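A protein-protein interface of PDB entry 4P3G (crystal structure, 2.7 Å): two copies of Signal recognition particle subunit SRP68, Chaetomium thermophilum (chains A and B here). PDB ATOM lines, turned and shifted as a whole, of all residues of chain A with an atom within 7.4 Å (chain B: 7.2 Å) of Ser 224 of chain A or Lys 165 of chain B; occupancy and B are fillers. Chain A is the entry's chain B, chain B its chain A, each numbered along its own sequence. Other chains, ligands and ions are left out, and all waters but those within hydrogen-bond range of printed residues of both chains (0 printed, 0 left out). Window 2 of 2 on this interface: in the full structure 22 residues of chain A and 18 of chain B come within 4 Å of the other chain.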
ATOM      1  N   ILE A 216     -22.921   2.908  -9.274  1.00  0.00           N
ATOM      2  CA  ILE A 216     -22.365   3.967  -8.444  1.00  0.00           C
ATOM      3  C   ILE A 216     -21.048   4.443  -9.012  1.00  0.00           C
ATOM      4  O   ILE A 216     -20.842   5.650  -9.203  1.00  0.00           O
ATOM      5  CB  ILE A 216     -22.181   3.495  -7.018  1.00  0.00           C
ATOM      6  CG1 ILE A 216     -23.535   3.470  -6.316  1.00  0.00           C
ATOM      7  CG2 ILE A 216     -21.301   4.456  -6.278  1.00  0.00           C
ATOM      8  CD1 ILE A 216     -23.592   2.515  -5.154  1.00  0.00           C
ATOM      9  N   ALA A 217     -20.176   3.481  -9.320  1.00  0.00           N
ATOM     10  CA  ALA A 217     -18.868   3.795  -9.880  1.00  0.00           C
ATOM     11  C   ALA A 217     -18.995   4.632 -11.148  1.00  0.00           C
ATOM     12  O   ALA A 217     -18.339   5.656 -11.282  1.00  0.00           O
ATOM     13  CB  ALA A 217     -18.096   2.540 -10.153  1.00  0.00           C
ATOM     14  N   ARG A 219     -21.601   6.526 -12.208  1.00  0.00           N
ATOM     15  CA  ARG A 219     -22.298   7.786 -11.983  1.00  0.00           C
ATOM     16  C   ARG A 219     -21.481   8.779 -11.132  1.00  0.00           C
ATOM     17  O   ARG A 219     -21.540   9.996 -11.346  1.00  0.00           O
ATOM     18  CB  ARG A 219     -23.673   7.528 -11.381  1.00  0.00           C
ATOM     19  CG  ARG A 219     -24.501   8.788 -11.220  1.00  0.00           C
ATOM     20  CD  ARG A 219     -24.678   9.501 -12.545  1.00  0.00           C
ATOM     21  NE  ARG A 219     -25.381   8.665 -13.511  1.00  0.00           N
ATOM     22  CZ  ARG A 219     -25.382   8.871 -14.825  1.00  0.00           C
ATOM     23  NH1 ARG A 219     -26.054   8.037 -15.609  1.00  0.00           N
ATOM     24  NH2 ARG A 219     -24.708   9.896 -15.351  1.00  0.00           N
ATOM     25  N   ALA A 220     -20.744   8.263 -10.152  1.00  0.00           N
ATOM     26  CA  ALA A 220     -19.896   9.115  -9.331  1.00  0.00           C
ATOM     27  C   ALA A 220     -18.880   9.877 -10.190  1.00  0.00           C
ATOM     28  O   ALA A 220     -18.664  11.059  -9.983  1.00  0.00           O
ATOM     29  CB  ALA A 220     -19.195   8.306  -8.271  1.00  0.00           C
ATOM     30  N   PHE A 221     -18.250   9.223 -11.153  1.00  0.00           N
ATOM     31  CA  PHE A 221     -17.264   9.938 -11.955  1.00  0.00           C
ATOM     32  C   PHE A 221     -17.876  10.833 -13.026  1.00  0.00           C
ATOM     33  O   PHE A 221     -17.282  11.843 -13.401  1.00  0.00           O
ATOM     34  CB  PHE A 221     -16.287   8.960 -12.616  1.00  0.00           C
ATOM     35  CG  PHE A 221     -15.348   8.316 -11.661  1.00  0.00           C
ATOM     36  CD1 PHE A 221     -15.758   7.240 -10.892  1.00  0.00           C
ATOM     37  CD2 PHE A 221     -14.066   8.804 -11.501  1.00  0.00           C
ATOM     38  CE1 PHE A 221     -14.899   6.646  -9.980  1.00  0.00           C
ATOM     39  CE2 PHE A 221     -13.204   8.226 -10.595  1.00  0.00           C
ATOM     40  CZ  PHE A 221     -13.622   7.141  -9.826  1.00  0.00           C
ATOM     41  N   GLU A 222     -19.080  10.501 -13.481  1.00  0.00           N
ATOM     42  CA  GLU A 222     -19.728  11.294 -14.517  1.00  0.00           C
ATOM     43  C   GLU A 222     -20.177  12.644 -13.961  1.00  0.00           C
ATOM     44  O   GLU A 222     -20.014  13.682 -14.602  1.00  0.00           O
ATOM     45  CB  GLU A 222     -20.915  10.521 -15.114  1.00  0.00           C
ATOM     46  CG  GLU A 222     -21.615  11.164 -16.333  1.00  0.00           C
ATOM     47  CD  GLU A 222     -20.837  11.018 -17.650  1.00  0.00           C
ATOM     48  OE1 GLU A 222     -19.891  10.197 -17.718  1.00  0.00           O
ATOM     49  OE2 GLU A 222     -21.194  11.714 -18.632  1.00  0.00           O
ATOM     50  N   GLN A 223     -20.712  12.617 -12.746  1.00  0.00           N
ATOM     51  CA  GLN A 223     -21.214  13.815 -12.073  1.00  0.00           C
ATOM     52  C   GLN A 223     -20.141  14.876 -11.734  1.00  0.00           C
ATOM     53  O   GLN A 223     -20.408  16.079 -11.803  1.00  0.00           O
ATOM     54  CB  GLN A 223     -21.989  13.394 -10.818  1.00  0.00           C
ATOM     55  CG  GLN A 223     -22.537  14.533  -9.973  1.00  0.00           C
ATOM     56  CD  GLN A 223     -23.363  14.037  -8.800  1.00  0.00           C
ATOM     57  OE1 GLN A 223     -23.622  12.838  -8.669  1.00  0.00           O
ATOM     58  NE2 GLN A 223     -23.752  14.952  -7.921  1.00  0.00           N
ATOM     59  N   SER A 224     -18.934  14.436 -11.379  1.00  0.00           N
ATOM     60  CA  SER A 224     -17.845  15.367 -11.070  1.00  0.00           C
ATOM     61  C   SER A 224     -16.955  15.611 -12.285  1.00  0.00           C
ATOM     62  O   SER A 224     -15.741  15.401 -12.225  1.00  0.00           O
ATOM     63  CB  SER A 224     -16.992  14.856  -9.900  1.00  0.00           C
ATOM     64  OG  SER A 224     -16.282  13.677 -10.241  1.00  0.00           O
ATOM     65  N   ALA B 147      -7.824   5.326   0.075  1.00  0.00           N
ATOM     66  CA  ALA B 147      -9.107   5.622  -0.544  1.00  0.00           C
ATOM     67  C   ALA B 147     -10.145   5.715   0.530  1.00  0.00           C
ATOM     68  O   ALA B 147     -11.053   6.532   0.450  1.00  0.00           O
ATOM     69  CB  ALA B 147      -9.475   4.559  -1.559  1.00  0.00           C
ATOM     70  N   GLY B 151     -12.317   8.863   1.348  1.00  0.00           N
ATOM     71  CA  GLY B 151     -13.757   8.708   1.347  1.00  0.00           C
ATOM     72  C   GLY B 151     -14.417   9.326   2.576  1.00  0.00           C
ATOM     73  O   GLY B 151     -15.435  10.013   2.458  1.00  0.00           O
ATOM     74  N   LEU B 154     -14.465  13.302   2.352  1.00  0.00           N
ATOM     75  CA  LEU B 154     -15.477  13.900   1.467  1.00  0.00           C
ATOM     76  C   LEU B 154     -16.898  13.616   1.957  1.00  0.00           C
ATOM     77  O   LEU B 154     -17.817  14.427   1.783  1.00  0.00           O
ATOM     78  CB  LEU B 154     -15.302  13.409   0.041  1.00  0.00           C
ATOM     79  CG  LEU B 154     -14.001  13.804  -0.657  1.00  0.00           C
ATOM     80  CD1 LEU B 154     -13.737  12.846  -1.819  1.00  0.00           C
ATOM     81  CD2 LEU B 154     -14.041  15.265  -1.111  1.00  0.00           C
ATOM     82  N   ASN B 159     -19.789  16.099   0.360  1.00  0.00           N
ATOM     83  CA  ASN B 159     -19.561  16.120  -1.072  1.00  0.00           C
ATOM     84  C   ASN B 159     -19.768  14.711  -1.608  1.00  0.00           C
ATOM     85  O   ASN B 159     -18.812  13.976  -1.834  1.00  0.00           O
ATOM     86  CB  ASN B 159     -18.152  16.636  -1.340  1.00  0.00           C
ATOM     87  CG  ASN B 159     -17.886  16.876  -2.801  1.00  0.00           C
ATOM     88  OD1 ASN B 159     -18.656  16.454  -3.676  1.00  0.00           O
ATOM     89  ND2 ASN B 159     -16.794  17.581  -3.083  1.00  0.00           N
ATOM     90  N   TRP B 160     -21.037  14.335  -1.776  1.00  0.00           N
ATOM     91  CA  TRP B 160     -21.431  12.939  -1.976  1.00  0.00           C
ATOM     92  C   TRP B 160     -20.865  12.239  -3.194  1.00  0.00           C
ATOM     93  O   TRP B 160     -20.459  11.086  -3.104  1.00  0.00           O
ATOM     94  CB  TRP B 160     -22.949  12.816  -1.984  1.00  0.00           C
ATOM     95  CG  TRP B 160     -23.591  13.499  -0.828  1.00  0.00           C
ATOM     96  CD1 TRP B 160     -24.445  14.554  -0.878  1.00  0.00           C
ATOM     97  CD2 TRP B 160     -23.405  13.202   0.561  1.00  0.00           C
ATOM     98  NE1 TRP B 160     -24.839  14.915   0.382  1.00  0.00           N
ATOM     99  CE2 TRP B 160     -24.202  14.110   1.294  1.00  0.00           C
ATOM    100  CE3 TRP B 160     -22.653  12.249   1.262  1.00  0.00           C
ATOM    101  CZ2 TRP B 160     -24.259  14.108   2.692  1.00  0.00           C
ATOM    102  CZ3 TRP B 160     -22.718  12.237   2.651  1.00  0.00           C
ATOM    103  CH2 TRP B 160     -23.531  13.154   3.345  1.00  0.00           C
ATOM    104  N   GLY B 161     -20.859  12.899  -4.341  1.00  0.00           N
ATOM    105  CA  GLY B 161     -20.337  12.243  -5.517  1.00  0.00           C
ATOM    106  C   GLY B 161     -18.871  11.873  -5.400  1.00  0.00           C
ATOM    107  O   GLY B 161     -18.503  10.709  -5.550  1.00  0.00           O
ATOM    108  N   ALA B 162     -18.046  12.849  -5.038  1.00  0.00           N
ATOM    109  CA  ALA B 162     -16.603  12.648  -4.982  1.00  0.00           C
ATOM    110  C   ALA B 162     -16.260  11.546  -4.007  1.00  0.00           C
ATOM    111  O   ALA B 162     -15.356  10.751  -4.239  1.00  0.00           O
ATOM    112  CB  ALA B 162     -15.920  13.930  -4.574  1.00  0.00           C
ATOM    113  N   CYS B 163     -17.000  11.516  -2.912  1.00  0.00           N
ATOM    114  CA  CYS B 163     -16.794  10.558  -1.839  1.00  0.00           C
ATOM    115  C   CYS B 163     -17.062   9.139  -2.349  1.00  0.00           C
ATOM    116  O   CYS B 163     -16.417   8.162  -1.927  1.00  0.00           O
ATOM    117  CB  CYS B 163     -17.684  10.935  -0.643  1.00  0.00           C
ATOM    118  SG  CYS B 163     -18.715   9.627   0.057  1.00  0.00           S
ATOM    119  N   LEU B 164     -18.052   9.035  -3.235  1.00  0.00           N
ATOM    120  CA  LEU B 164     -18.417   7.763  -3.826  1.00  0.00           C
ATOM    121  C   LEU B 164     -17.296   7.274  -4.710  1.00  0.00           C
ATOM    122  O   LEU B 164     -17.054   6.071  -4.780  1.00  0.00           O
ATOM    123  CB  LEU B 164     -19.722   7.863  -4.591  1.00  0.00           C
ATOM    124  CG  LEU B 164     -20.894   7.894  -3.640  1.00  0.00           C
ATOM    125  CD1 LEU B 164     -22.191   8.060  -4.412  1.00  0.00           C
ATOM    126  CD2 LEU B 164     -20.902   6.617  -2.864  1.00  0.00           C
ATOM    127  N   LYS B 165     -16.606   8.203  -5.372  1.00  0.00           N
ATOM    128  CA  LYS B 165     -15.451   7.816  -6.193  1.00  0.00           C
ATOM    129  C   LYS B 165     -14.384   7.170  -5.328  1.00  0.00           C
ATOM    130  O   LYS B 165     -13.833   6.146  -5.715  1.00  0.00           O
ATOM    131  CB  LYS B 165     -14.838   8.991  -6.961  1.00  0.00           C
ATOM    132  CG  LYS B 165     -15.835   9.839  -7.673  1.00  0.00           C
ATOM    133  CD  LYS B 165     -15.170  10.641  -8.774  1.00  0.00           C
ATOM    134  CE  LYS B 165     -14.330  11.760  -8.223  1.00  0.00           C
ATOM    135  NZ  LYS B 165     -14.099  12.786  -9.273  1.00  0.00           N
ATOM    136  N   SER B 166     -14.084   7.755  -4.166  1.00  0.00           N
ATOM    137  CA  SER B 166     -13.054   7.165  -3.303  1.00  0.00           C
ATOM    138  C   SER B 166     -13.455   5.818  -2.763  1.00  0.00           C
ATOM    139  O   SER B 166     -12.686   4.861  -2.825  1.00  0.00           O
ATOM    140  CB  SER B 166     -12.707   8.062  -2.127  1.00  0.00           C
ATOM    141  OG  SER B 166     -11.957   9.161  -2.564  1.00  0.00           O
ATOM    142  N   TYR B 167     -14.674   5.744  -2.249  1.00  0.00           N
ATOM    143  CA  TYR B 167     -15.153   4.523  -1.628  1.00  0.00           C
ATOM    144  C   TYR B 167     -15.262   3.376  -2.624  1.00  0.00           C
ATOM    145  O   TYR B 167     -15.077   2.201  -2.265  1.00  0.00           O
ATOM    146  CB  TYR B 167     -16.503   4.785  -0.964  1.00  0.00           C
ATOM    147  CG  TYR B 167     -16.429   5.354   0.425  1.00  0.00           C
ATOM    148  CD1 TYR B 167     -15.606   4.789   1.385  1.00  0.00           C
ATOM    149  CD2 TYR B 167     -17.165   6.475   0.770  1.00  0.00           C
ATOM    150  CE1 TYR B 167     -15.540   5.295   2.661  1.00  0.00           C
ATOM    151  CE2 TYR B 167     -17.104   7.008   2.056  1.00  0.00           C
ATOM    152  CZ  TYR B 167     -16.290   6.412   3.000  1.00  0.00           C
ATOM    153  OH  TYR B 167     -16.219   6.941   4.280  1.00  0.00           O
ATOM    154  N   ALA B 168     -15.558   3.715  -3.878  1.00  0.00           N
ATOM    155  CA  ALA B 168     -15.642   2.696  -4.906  1.00  0.00           C
ATOM    156  C   ALA B 168     -14.267   2.073  -5.076  1.00  0.00           C
ATOM    157  O   ALA B 168     -14.150   0.841  -5.097  1.00  0.00           O
ATOM    158  CB  ALA B 168     -16.143   3.276  -6.215  1.00  0.00           C
ATOM    159  N   ILE B 169     -13.222   2.909  -5.140  1.00  0.00           N
ATOM    160  CA  ILE B 169     -11.879   2.367  -5.287  1.00  0.00           C
ATOM    161  C   ILE B 169     -11.579   1.405  -4.122  1.00  0.00           C
ATOM    162  O   ILE B 169     -11.202   0.260  -4.348  1.00  0.00           O
ATOM    163  CB  ILE B 169     -10.774   3.435  -5.293  1.00  0.00           C
ATOM    164  CG1 ILE B 169     -10.956   4.487  -6.382  1.00  0.00           C
ATOM    165  CG2 ILE B 169      -9.408   2.783  -5.303  1.00  0.00           C
ATOM    166  CD1 ILE B 169     -10.969   3.935  -7.696  1.00  0.00           C
ATOM    167  N   CYS B 170     -11.764   1.836  -2.872  1.00  0.00           N
ATOM    168  CA  CYS B 170     -11.336   0.953  -1.788  1.00  0.00           C
ATOM    169  C   CYS B 170     -12.206  -0.288  -1.617  1.00  0.00           C
ATOM    170  O   CYS B 170     -11.712  -1.362  -1.257  1.00  0.00           O
ATOM    171  CB  CYS B 170     -11.175   1.669  -0.436  1.00  0.00           C
ATOM    172  SG  CYS B 170     -12.641   2.093   0.454  1.00  0.00           S
ATOM    173  N   MET B 198     -21.401   4.097   1.695  1.00  0.00           N
ATOM    174  CA  MET B 198     -21.719   4.211   0.299  1.00  0.00           C
ATOM    175  C   MET B 198     -23.228   4.263   0.118  1.00  0.00           C
ATOM    176  O   MET B 198     -23.729   5.092  -0.643  1.00  0.00           O
ATOM    177  CB  MET B 198     -21.138   3.040  -0.458  1.00  0.00           C
ATOM    178  CG  MET B 198     -19.618   3.055  -0.514  1.00  0.00           C
ATOM    179  SD  MET B 198     -18.985   1.808  -1.874  1.00  0.00           S
ATOM    180  CE  MET B 198     -19.217   3.002  -3.411  1.00  0.00           C
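The side-chain amino group (NZ) of Lys 165 of chain B lies within hydrogen-bond range of the side-chain hydroxyl (OG) of Ser 224 of chain A, at 2.5 Å.
Ile 216 of chain A touches Met 198 of chain B (CG2 to CE, 3.8 Å). Ala 220 of chain A touches Gly 161 of chain B. Leu 164 of chain B touches Ala 220 of chain A (CB to CB, 3.7 Å). O of Ala 220 of chain A touches CD of Lys 165 of chain B, at 3.7 Å. Lys 165 of chain B touches Phe 221 of chain A.
Lys 165 of chain B touches just these residues of chain A: Ala 220 (3.7 Å), Phe 221 (3.5 Å) and Ser 224 (2.5 Å). Printed residues of chain A within 4 Å of Met 198 of chain B: Ile 216. Printed residues of chain B within 4 Å of Ile 216 of chain A: Met 198 (3.8 Å). Of the printed residues of chain A, Gly 161 of chain B touches Ala 220. Of the printed residues of chain B, Phe 221 of chain A touches Lys 165 (3.5 Å). Glu 222 of chain A touches none of the printed residues of chain B. The nearest residue of chain B that does not touch Ser 224 of chain A is Ala 162 of chain B (5.4 Å). The nearest printed residue of chain B that does not touch Ile 216 of chain A is Leu 164 of chain B (4.1 Å).
Printed residues of chain B that touch a printed residue of chain A: Gly 161, Leu 164, Lys 165 and Met 198. Among the printed residues, 6 pairs touch across the chains. Among the printed residues, no Asp or Glu carboxylate lies within 4 Å of a Lys or Arg side-chain nitrogen of the other chain.
No position is printed for both chains. Of the 6 pairs that touch across the chains among the printed residues, none has its exchanged pair printed and touching as well.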
